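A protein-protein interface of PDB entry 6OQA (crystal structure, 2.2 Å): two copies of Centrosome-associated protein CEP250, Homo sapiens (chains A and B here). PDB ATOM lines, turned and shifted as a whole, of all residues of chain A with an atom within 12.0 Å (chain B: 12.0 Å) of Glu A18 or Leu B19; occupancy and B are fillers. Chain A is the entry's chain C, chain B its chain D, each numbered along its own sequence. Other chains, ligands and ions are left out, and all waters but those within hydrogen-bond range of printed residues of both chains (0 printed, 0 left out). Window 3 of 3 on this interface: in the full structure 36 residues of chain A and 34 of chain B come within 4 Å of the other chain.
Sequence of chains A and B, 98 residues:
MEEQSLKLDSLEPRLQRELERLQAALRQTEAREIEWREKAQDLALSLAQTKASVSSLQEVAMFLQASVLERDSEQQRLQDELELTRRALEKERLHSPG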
ATOM      1  N   PRO A  13      33.105 -13.897  25.848  1.00  0.00           N
ATOM      2  CA  PRO A  13      31.831 -14.462  25.398  1.00  0.00           C
ATOM      3  C   PRO A  13      31.106 -13.588  24.364  1.00  0.00           C
ATOM      4  O   PRO A  13      31.668 -12.600  23.883  1.00  0.00           O
ATOM      5  CB  PRO A  13      31.010 -14.580  26.704  1.00  0.00           C
ATOM      6  CG  PRO A  13      31.932 -14.195  27.819  1.00  0.00           C
ATOM      7  CD  PRO A  13      32.996 -13.343  27.203  1.00  0.00           C
ATOM      8  N   ARG A  14      29.872 -13.965  24.038  1.00  0.00           N
ATOM      9  CA  ARG A  14      29.037 -13.237  23.074  1.00  0.00           C
ATOM     10  C   ARG A  14      28.213 -12.162  23.786  1.00  0.00           C
ATOM     11  O   ARG A  14      28.177 -11.006  23.357  1.00  0.00           O
ATOM     12  CB  ARG A  14      28.085 -14.199  22.354  1.00  0.00           C
ATOM     13  CG  ARG A  14      28.743 -15.434  21.738  1.00  0.00           C
ATOM     14  CD  ARG A  14      27.730 -16.548  21.472  1.00  0.00           C
ATOM     15  NE  ARG A  14      28.195 -17.854  21.948  1.00  0.00           N
ATOM     16  CZ  ARG A  14      27.444 -18.955  22.042  1.00  0.00           C
ATOM     17  NH1 ARG A  14      26.155 -18.955  21.691  1.00  0.00           N
ATOM     18  NH2 ARG A  14      27.991 -20.082  22.497  1.00  0.00           N
ATOM     19  N   LEU A  15      27.557 -12.563  24.877  1.00  0.00           N
ATOM     20  CA  LEU A  15      26.604 -11.712  25.604  1.00  0.00           C
ATOM     21  C   LEU A  15      27.245 -10.694  26.560  1.00  0.00           C
ATOM     22  O   LEU A  15      26.630  -9.665  26.844  1.00  0.00           O
ATOM     23  CB  LEU A  15      25.604 -12.584  26.379  1.00  0.00           C
ATOM     24  N   GLN A  16      28.455 -10.978  27.054  1.00  0.00           N
ATOM     25  CA  GLN A  16      29.168 -10.069  27.977  1.00  0.00           C
ATOM     26  C   GLN A  16      29.423  -8.677  27.381  1.00  0.00           C
ATOM     27  O   GLN A  16      29.421  -7.678  28.108  1.00  0.00           O
ATOM     28  CB  GLN A  16      30.501 -10.679  28.437  1.00  0.00           C
ATOM     29  CG  GLN A  16      31.149  -9.943  29.608  1.00  0.00           C
ATOM     30  CD  GLN A  16      32.478 -10.540  30.031  1.00  0.00           C
ATOM     31  OE1 GLN A  16      33.318 -10.875  29.196  1.00  0.00           O
ATOM     32  NE2 GLN A  16      32.683 -10.654  31.338  1.00  0.00           N
ATOM     33  N   ARG A  17      29.649  -8.621  26.070  1.00  0.00           N
ATOM     34  CA  ARG A  17      29.835  -7.353  25.357  1.00  0.00           C
ATOM     35  C   ARG A  17      28.533  -6.549  25.311  1.00  0.00           C
ATOM     36  O   ARG A  17      28.543  -5.337  25.536  1.00  0.00           O
ATOM     37  CB  ARG A  17      30.331  -7.611  23.933  1.00  0.00           C
ATOM     38  CG  ARG A  17      30.897  -6.394  23.211  1.00  0.00           C
ATOM     39  CD  ARG A  17      30.840  -6.580  21.701  1.00  0.00           C
ATOM     40  NE  ARG A  17      31.390  -7.874  21.287  1.00  0.00           N
ATOM     41  CZ  ARG A  17      31.208  -8.452  20.096  1.00  0.00           C
ATOM     42  NH1 ARG A  17      30.482  -7.870  19.138  1.00  0.00           N
ATOM     43  NH2 ARG A  17      31.767  -9.636  19.858  1.00  0.00           N
ATOM     44  N   GLU A  18      27.428  -7.233  25.012  1.00  0.00           N
ATOM     45  CA  GLU A  18      26.105  -6.601  24.948  1.00  0.00           C
ATOM     46  C   GLU A  18      25.567  -6.239  26.340  1.00  0.00           C
ATOM     47  O   GLU A  18      24.854  -5.244  26.483  1.00  0.00           O
ATOM     48  CB  GLU A  18      25.105  -7.507  24.214  1.00  0.00           C
ATOM     49  CG  GLU A  18      23.816  -6.819  23.767  1.00  0.00           C
ATOM     50  CD  GLU A  18      24.042  -5.715  22.742  1.00  0.00           C
ATOM     51  OE1 GLU A  18      24.892  -5.889  21.841  1.00  0.00           O
ATOM     52  OE2 GLU A  18      23.365  -4.667  22.834  1.00  0.00           O
ATOM     53  N   LEU A  19      25.900  -7.049  27.348  1.00  0.00           N
ATOM     54  CA  LEU A  19      25.566  -6.742  28.746  1.00  0.00           C
ATOM     55  C   LEU A  19      26.281  -5.476  29.217  1.00  0.00           C
ATOM     56  O   LEU A  19      25.654  -4.607  29.820  1.00  0.00           O
ATOM     57  CB  LEU A  19      25.904  -7.922  29.668  1.00  0.00           C
ATOM     58  CG  LEU A  19      25.541  -7.760  31.155  1.00  0.00           C
ATOM     59  CD1 LEU A  19      24.918  -9.029  31.720  1.00  0.00           C
ATOM     60  CD2 LEU A  19      26.749  -7.347  31.989  1.00  0.00           C
ATOM     61  N   GLU A  20      27.582  -5.381  28.931  1.00  0.00           N
ATOM     62  CA  GLU A  20      28.368  -4.166  29.208  1.00  0.00           C
ATOM     63  C   GLU A  20      27.851  -2.943  28.438  1.00  0.00           C
ATOM     64  O   GLU A  20      27.829  -1.835  28.978  1.00  0.00           O
ATOM     65  CB  GLU A  20      29.854  -4.386  28.891  1.00  0.00           C
ATOM     66  CG  GLU A  20      30.582  -5.257  29.902  1.00  0.00           C
ATOM     67  N   ARG A  21      27.441  -3.152  27.188  1.00  0.00           N
ATOM     68  CA  ARG A  21      26.872  -2.078  26.364  1.00  0.00           C
ATOM     69  C   ARG A  21      25.495  -1.625  26.870  1.00  0.00           C
ATOM     70  O   ARG A  21      25.184  -0.438  26.816  1.00  0.00           O
ATOM     71  CB  ARG A  21      26.785  -2.500  24.888  1.00  0.00           C
ATOM     72  CG  ARG A  21      26.531  -1.336  23.935  1.00  0.00           C
ATOM     73  CD  ARG A  21      26.868  -1.661  22.484  1.00  0.00           C
ATOM     74  NE  ARG A  21      25.733  -2.212  21.740  1.00  0.00           N
ATOM     75  CZ  ARG A  21      24.718  -1.507  21.231  1.00  0.00           C
ATOM     76  NH1 ARG A  21      24.638  -0.182  21.383  1.00  0.00           N
ATOM     77  NH2 ARG A  21      23.755  -2.140  20.562  1.00  0.00           N
ATOM     78  N   LEU A  22      24.687  -2.569  27.355  1.00  0.00           N
ATOM     79  CA  LEU A  22      23.367  -2.258  27.921  1.00  0.00           C
ATOM     80  C   LEU A  22      23.459  -1.590  29.299  1.00  0.00           C
ATOM     81  O   LEU A  22      22.641  -0.726  29.618  1.00  0.00           O
ATOM     82  CB  LEU A  22      22.482  -3.510  27.999  1.00  0.00           C
ATOM     83  CG  LEU A  22      21.795  -3.944  26.700  1.00  0.00           C
ATOM     84  CD1 LEU A  22      21.149  -5.307  26.883  1.00  0.00           C
ATOM     85  CD2 LEU A  22      20.750  -2.931  26.254  1.00  0.00           C
ATOM     86  N   GLN A  23      24.431  -2.010  30.109  1.00  0.00           N
ATOM     87  CA  GLN A  23      24.723  -1.361  31.395  1.00  0.00           C
ATOM     88  C   GLN A  23      25.128   0.103  31.203  1.00  0.00           C
ATOM     89  O   GLN A  23      24.621   0.977  31.905  1.00  0.00           O
ATOM     90  CB  GLN A  23      25.829  -2.107  32.155  1.00  0.00           C
ATOM     91  CG  GLN A  23      25.358  -3.358  32.888  1.00  0.00           C
ATOM     92  CD  GLN A  23      26.474  -4.043  33.658  1.00  0.00           C
ATOM     93  OE1 GLN A  23      27.646  -3.973  33.277  1.00  0.00           O
ATOM     94  NE2 GLN A  23      26.116  -4.707  34.754  1.00  0.00           N
ATOM     95  N   ALA A  24      26.025   0.351  30.249  1.00  0.00           N
ATOM     96  CA  ALA A  24      26.522   1.706  29.955  1.00  0.00           C
ATOM     97  C   ALA A  24      25.447   2.634  29.391  1.00  0.00           C
ATOM     98  O   ALA A  24      25.361   3.797  29.787  1.00  0.00           O
ATOM     99  CB  ALA A  24      27.705   1.647  28.998  1.00  0.00           C
ATOM    100  N   ALA A  25      24.646   2.119  28.461  1.00  0.00           N
ATOM    101  CA  ALA A  25      23.520   2.867  27.893  1.00  0.00           C
ATOM    102  C   ALA A  25      22.454   3.213  28.941  1.00  0.00           C
ATOM    103  O   ALA A  25      21.926   4.322  28.934  1.00  0.00           O
ATOM    104  CB  ALA A  25      22.889   2.090  26.748  1.00  0.00           C
ATOM    105  N   LEU A  26      22.149   2.270  29.834  1.00  0.00           N
ATOM    106  CA  LEU A  26      21.134   2.476  30.874  1.00  0.00           C
ATOM    107  C   LEU A  26      21.561   3.538  31.904  1.00  0.00           C
ATOM    108  O   LEU A  26      20.776   4.436  32.218  1.00  0.00           O
ATOM    109  CB  LEU A  26      20.798   1.158  31.577  1.00  0.00           C
ATOM    110  CG  LEU A  26      19.615   1.137  32.551  1.00  0.00           C
ATOM    111  CD1 LEU A  26      18.303   1.463  31.850  1.00  0.00           C
ATOM    112  CD2 LEU A  26      19.514  -0.212  33.251  1.00  0.00           C
ATOM    113  N   ARG A  27      22.793   3.440  32.405  1.00  0.00           N
ATOM    114  CA  ARG A  27      23.297   4.383  33.420  1.00  0.00           C
ATOM    115  C   ARG A  27      23.458   5.803  32.875  1.00  0.00           C
ATOM    116  O   ARG A  27      23.179   6.765  33.585  1.00  0.00           O
ATOM    117  CB  ARG A  27      24.602   3.890  34.078  1.00  0.00           C
ATOM    118  CG  ARG A  27      25.858   3.938  33.222  1.00  0.00           C
ATOM    119  CD  ARG A  27      27.078   3.426  33.981  1.00  0.00           C
ATOM    120  NE  ARG A  27      28.147   3.000  33.071  1.00  0.00           N
ATOM    121  CZ  ARG A  27      29.271   2.373  33.431  1.00  0.00           C
ATOM    122  NH1 ARG A  27      29.530   2.079  34.707  1.00  0.00           N
ATOM    123  NH2 ARG A  27      30.158   2.038  32.496  1.00  0.00           N
ATOM    124  N   GLN A  28      23.910   5.918  31.625  1.00  0.00           N
ATOM    125  CA  GLN A  28      24.028   7.214  30.946  1.00  0.00           C
ATOM    126  C   GLN A  28      22.667   7.863  30.705  1.00  0.00           C
ATOM    127  O   GLN A  28      22.519   9.068  30.888  1.00  0.00           O
ATOM    128  CB  GLN A  28      24.773   7.073  29.613  1.00  0.00           C
ATOM    129  CG  GLN A  28      26.278   6.893  29.768  1.00  0.00           C
ATOM    130  CD  GLN A  28      26.954   6.370  28.509  1.00  0.00           C
ATOM    131  OE1 GLN A  28      26.369   6.364  27.422  1.00  0.00           O
ATOM    132  NE2 GLN A  28      28.196   5.927  28.655  1.00  0.00           N
ATOM    133  N   PRO B  13      22.255 -19.745  28.239  1.00  0.00           N
ATOM    134  CA  PRO B  13      20.889 -20.261  28.263  1.00  0.00           C
ATOM    135  C   PRO B  13      19.875 -19.260  28.840  1.00  0.00           C
ATOM    136  O   PRO B  13      18.978 -18.821  28.117  1.00  0.00           O
ATOM    137  CB  PRO B  13      21.003 -21.529  29.130  1.00  0.00           C
ATOM    138  CG  PRO B  13      22.303 -21.414  29.872  1.00  0.00           C
ATOM    139  CD  PRO B  13      23.027 -20.179  29.413  1.00  0.00           C
ATOM    140  N   ARG B  14      20.031 -18.906  30.117  1.00  0.00           N
ATOM    141  CA  ARG B  14      19.176 -17.900  30.779  1.00  0.00           C
ATOM    142  C   ARG B  14      19.636 -16.450  30.543  1.00  0.00           C
ATOM    143  O   ARG B  14      18.890 -15.511  30.837  1.00  0.00           O
ATOM    144  CB  ARG B  14      19.054 -18.178  32.292  1.00  0.00           C
ATOM    145  CG  ARG B  14      20.361 -18.172  33.081  1.00  0.00           C
ATOM    146  CD  ARG B  14      20.112 -18.138  34.582  1.00  0.00           C
ATOM    147  NE  ARG B  14      19.645 -16.829  35.046  1.00  0.00           N
ATOM    148  CZ  ARG B  14      20.405 -15.739  35.202  1.00  0.00           C
ATOM    149  NH1 ARG B  14      21.710 -15.751  34.920  1.00  0.00           N
ATOM    150  NH2 ARG B  14      19.849 -14.611  35.637  1.00  0.00           N
ATOM    151  N   LEU B  15      20.853 -16.274  30.022  1.00  0.00           N
ATOM    152  CA  LEU B  15      21.427 -14.943  29.775  1.00  0.00           C
ATOM    153  C   LEU B  15      20.788 -14.212  28.589  1.00  0.00           C
ATOM    154  O   LEU B  15      20.845 -12.983  28.523  1.00  0.00           O
ATOM    155  CB  LEU B  15      22.942 -15.042  29.559  1.00  0.00           C
ATOM    156  N   GLN B  16      20.200 -14.964  27.656  1.00  0.00           N
ATOM    157  CA  GLN B  16      19.421 -14.384  26.550  1.00  0.00           C
ATOM    158  C   GLN B  16      18.155 -13.662  27.033  1.00  0.00           C
ATOM    159  O   GLN B  16      17.740 -12.666  26.432  1.00  0.00           O
ATOM    160  CB  GLN B  16      19.032 -15.466  25.537  1.00  0.00           C
ATOM    161  N   ARG B  17      17.555 -14.169  28.115  1.00  0.00           N
ATOM    162  CA  ARG B  17      16.333 -13.593  28.694  1.00  0.00           C
ATOM    163  C   ARG B  17      16.595 -12.237  29.358  1.00  0.00           C
ATOM    164  O   ARG B  17      15.862 -11.272  29.116  1.00  0.00           O
ATOM    165  CB  ARG B  17      15.716 -14.549  29.729  1.00  0.00           C
ATOM    166  CG  ARG B  17      15.305 -15.912  29.187  1.00  0.00           C
ATOM    167  N   GLU B  18      17.639 -12.175  30.188  1.00  0.00           N
ATOM    168  CA  GLU B  18      17.985 -10.959  30.950  1.00  0.00           C
ATOM    169  C   GLU B  18      18.434  -9.784  30.074  1.00  0.00           C
ATOM    170  O   GLU B  18      18.165  -8.628  30.403  1.00  0.00           O
ATOM    171  CB  GLU B  18      19.074 -11.262  31.989  1.00  0.00           C
ATOM    172  CG  GLU B  18      18.655 -12.237  33.083  1.00  0.00           C
ATOM    173  CD  GLU B  18      17.545 -11.702  33.973  1.00  0.00           C
ATOM    174  OE1 GLU B  18      16.563 -12.439  34.206  1.00  0.00           O
ATOM    175  OE2 GLU B  18      17.647 -10.545  34.434  1.00  0.00           O
ATOM    176  N   LEU B  19      19.128 -10.089  28.978  1.00  0.00           N
ATOM    177  CA  LEU B  19      19.510  -9.087  27.969  1.00  0.00           C
ATOM    178  C   LEU B  19      18.284  -8.397  27.344  1.00  0.00           C
ATOM    179  O   LEU B  19      18.309  -7.187  27.107  1.00  0.00           O
ATOM    180  CB  LEU B  19      20.377  -9.738  26.881  1.00  0.00           C
ATOM    181  CG  LEU B  19      21.037  -8.839  25.826  1.00  0.00           C
ATOM    182  CD1 LEU B  19      22.346  -9.446  25.338  1.00  0.00           C
ATOM    183  CD2 LEU B  19      20.113  -8.569  24.645  1.00  0.00           C
ATOM    184  N   GLU B  20      17.227  -9.170  27.083  1.00  0.00           N
ATOM    185  CA  GLU B  20      15.950  -8.629  26.584  1.00  0.00           C
ATOM    186  C   GLU B  20      15.205  -7.798  27.637  1.00  0.00           C
ATOM    187  O   GLU B  20      14.558  -6.804  27.297  1.00  0.00           O
ATOM    188  CB  GLU B  20      15.037  -9.755  26.075  1.00  0.00           C
ATOM    189  CG  GLU B  20      15.551 -10.470  24.834  1.00  0.00           C
ATOM    190  N   ARG B  21      15.286  -8.215  28.902  1.00  0.00           N
ATOM    191  CA  ARG B  21      14.680  -7.471  30.020  1.00  0.00           C
ATOM    192  C   ARG B  21      15.312  -6.084  30.174  1.00  0.00           C
ATOM    193  O   ARG B  21      14.601  -5.089  30.354  1.00  0.00           O
ATOM    194  CB  ARG B  21      14.822  -8.258  31.333  1.00  0.00           C
ATOM    195  CG  ARG B  21      13.997  -7.725  32.498  1.00  0.00           C
ATOM    196  N   LEU B  22      16.641  -6.034  30.091  1.00  0.00           N
ATOM    197  CA  LEU B  22      17.398  -4.787  30.244  1.00  0.00           C
ATOM    198  C   LEU B  22      17.191  -3.844  29.054  1.00  0.00           C
ATOM    199  O   LEU B  22      17.188  -2.622  29.227  1.00  0.00           O
ATOM    200  CB  LEU B  22      18.892  -5.088  30.444  1.00  0.00           C
ATOM    201  CG  LEU B  22      19.741  -4.029  31.147  1.00  0.00           C
ATOM    202  CD1 LEU B  22      19.256  -3.795  32.570  1.00  0.00           C
ATOM    203  CD2 LEU B  22      21.200  -4.456  31.153  1.00  0.00           C
ATOM    204  N   GLN B  23      17.033  -4.415  27.858  1.00  0.00           N
ATOM    205  CA  GLN B  23      16.618  -3.655  26.667  1.00  0.00           C
ATOM    206  C   GLN B  23      15.269  -2.952  26.877  1.00  0.00           C
ATOM    207  O   GLN B  23      15.115  -1.797  26.501  1.00  0.00           O
ATOM    208  CB  GLN B  23      16.535  -4.565  25.432  1.00  0.00           C
ATOM    209  CG  GLN B  23      17.876  -4.839  24.758  1.00  0.00           C
ATOM    210  CD  GLN B  23      17.811  -5.882  23.643  1.00  0.00           C
ATOM    211  OE1 GLN B  23      18.836  -6.227  23.055  1.00  0.00           O
ATOM    212  NE2 GLN B  23      16.613  -6.383  23.345  1.00  0.00           N
ATOM    213  N   ALA B  24      14.310  -3.657  27.477  1.00  0.00           N
ATOM    214  CA  ALA B  24      12.991  -3.089  27.793  1.00  0.00           C
ATOM    215  C   ALA B  24      13.043  -2.060  28.929  1.00  0.00           C
ATOM    216  O   ALA B  24      12.261  -1.105  28.934  1.00  0.00           O
ATOM    217  CB  ALA B  24      12.001  -4.195  28.133  1.00  0.00           C
ATOM    218  N   ALA B  25      13.944  -2.268  29.891  1.00  0.00           N
ATOM    219  CA  ALA B  25      14.201  -1.282  30.953  1.00  0.00           C
ATOM    220  C   ALA B  25      14.845  -0.006  30.394  1.00  0.00           C
ATOM    221  O   ALA B  25      14.555   1.093  30.864  1.00  0.00           O
ATOM    222  CB  ALA B  25      15.075  -1.882  32.049  1.00  0.00           C
ATOM    223  N   LEU B  26      15.713  -0.166  29.395  1.00  0.00           N
ATOM    224  CA  LEU B  26      16.330   0.963  28.699  1.00  0.00           C
ATOM    225  C   LEU B  26      15.317   1.780  27.893  1.00  0.00           C
ATOM    226  O   LEU B  26      15.421   3.004  27.847  1.00  0.00           O
ATOM    227  CB  LEU B  26      17.464   0.478  27.781  1.00  0.00           C
ATOM    228  CG  LEU B  26      18.158   1.500  26.875  1.00  0.00           C
ATOM    229  CD1 LEU B  26      18.667   2.683  27.684  1.00  0.00           C
ATOM    230  CD2 LEU B  26      19.292   0.840  26.108  1.00  0.00           C
ATOM    231  N   ARG B  27      14.362   1.106  27.247  1.00  0.00           N
ATOM    232  CA  ARG B  27      13.300   1.786  26.482  1.00  0.00           C
ATOM    233  C   ARG B  27      12.392   2.608  27.401  1.00  0.00           C
ATOM    234  O   ARG B  27      12.018   3.733  27.066  1.00  0.00           O
ATOM    235  CB  ARG B  27      12.440   0.783  25.696  1.00  0.00           C
ATOM    236  CG  ARG B  27      13.161  -0.005  24.607  1.00  0.00           C
ATOM    237  CD  ARG B  27      13.588   0.837  23.411  1.00  0.00           C
ATOM    238  NE  ARG B  27      14.960   1.348  23.517  1.00  0.00           N
ATOM    239  CZ  ARG B  27      16.078   0.624  23.376  1.00  0.00           C
ATOM    240  NH1 ARG B  27      16.033  -0.690  23.145  1.00  0.00           N
ATOM    241  NH2 ARG B  27      17.263   1.222  23.483  1.00  0.00           N
ATOM    242  N   GLN B  28      12.041   2.023  28.549  1.00  0.00           N
ATOM    243  CA  GLN B  28      11.250   2.696  29.591  1.00  0.00           C
ATOM    244  C   GLN B  28      11.949   3.966  30.103  1.00  0.00           C
ATOM    245  O   GLN B  28      11.311   5.010  30.239  1.00  0.00           O
ATOM    246  CB  GLN B  28      10.994   1.729  30.759  1.00  0.00           C
ATOM    247  CG  GLN B  28       9.999   2.203  31.818  1.00  0.00           C
ATOM    248  CD  GLN B  28       9.986   1.325  33.064  1.00  0.00           C
ATOM    249  OE1 GLN B  28      10.921   0.559  33.318  1.00  0.00           O
ATOM    250  NE2 GLN B  28       8.922   1.436  33.853  1.00  0.00           N
ATOM    251  N   GLU B  30      14.419   5.614  28.527  1.00  0.00           N
ATOM    252  CA  GLU B  30      14.457   6.514  27.367  1.00  0.00           C
ATOM    253  C   GLU B  30      13.161   7.315  27.216  1.00  0.00           C
ATOM    254  O   GLU B  30      13.197   8.499  26.885  1.00  0.00           O
ATOM    255  CB  GLU B  30      14.761   5.741  26.076  1.00  0.00           C
ATOM    256  CG  GLU B  30      16.244   5.487  25.843  1.00  0.00           C
ATOM    257  CD  GLU B  30      16.534   4.740  24.544  1.00  0.00           C
ATOM    258  OE1 GLU B  30      15.666   4.712  23.645  1.00  0.00           O
ATOM    259  OE2 GLU B  30      17.646   4.183  24.409  1.00  0.00           O
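The side-chain carboxylate (OE2) of Glu A18 lies within salt-bridge range of the guanidinium group (NH2) of Arg A21, 3.4 Å away.
Among the printed residues, pairs that only touch across the chains: Glu A18 with Leu B19, Leu A22 with Leu B19, Leu A22 with Leu B22, Leu A22 with Gln B23, Ala A25 with Leu B26, Leu A26 with Leu B22, Leu A26 with Ala B25 and Leu A26 with Leu B26.
No residue of chain B comes within 4 Å of Leu A15.
No residue of chain B comes within 4 Å of Arg A17.
Glu A18 touches just one residue of chain B: Leu B19 (3.4 Å).
No residue of chain B comes within 4 Å of Leu A19.
No residue of chain B comes within 4 Å of Glu A20.
Leu A22 touches just these residues of chain B: Leu B19, Leu B22 and Gln B23.
Of the printed residues of chain B, Leu A26 touches Leu B22 (3.7 Å), Ala B25 (3.9 Å) and Leu B26 (3.8 Å).
Arg A27 touches none of the printed residues of chain B.
No residue of chain A comes within 4 Å of Leu B15.
No residue of chain A comes within 4 Å of Glu B18.
Of chain A, only Glu A18 and Leu A22 come within 4 Å of Leu B19.
Glu B20 touches none of the printed residues of chain A.
No residue of chain A comes within 4 Å of Arg B21.
Of chain A, only Leu A22 (3.5 Å) and Leu A26 (3.7 Å) come within 4 Å of Leu B22.
Of chain A, only Leu A22 (3.8 Å) comes within 4 Å of Gln B23.
Of the printed residues of chain A, Ala B25 touches Leu A26 (3.9 Å).
The nearest residue of chain B that does not touch Glu A18 is Gln B23 (4.8 Å).
The nearest residue of chain A that does not touch Leu B19 is Leu A15 (4.5 Å).
The nearest printed residue of chain A that does not touch Leu B26 is Leu A22 (4.05 Å).
Of the 16 printed residues of chain A, 4 touch a printed residue of chain B.
Printed residues of chain A that touch a printed residue of chain B: Glu A18, Leu A22, Ala A25 and Leu A26.
Hydrophobic or aromatic side chains of chain A that line the printed part of chain B: Leu A22, Ala A25 and Leu A26.
Of the 17 printed residues of chain B, 5 touch a printed residue of chain A.
Printed residues of chain B that touch a printed residue of chain A: Leu B19, Leu B22, Gln B23, Ala B25 and Leu B26.
Glu A18 touches Leu B19, but with the chains exchanged Leu A19 does not touch Glu B18 (6.3 Å).
Ala A25 touches Leu B26, and with the chains exchanged Leu A26 touches Ala B25.
Leu A26 touches Leu B22, but with the chains exchanged Leu A22 does not touch Leu B26 (4.05 Å).
Leu B26 touches its own counterpart, Leu A26.
Positions printed for both chains: 13, 14, 15, 16, 17, 18, 19, 20, 21, 22, 23, 24, 25, 26, 27 and 28.
Of the 8 pairs that touch across the chains among the printed residues, 4 have their exchanged pair printed and touching as well.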
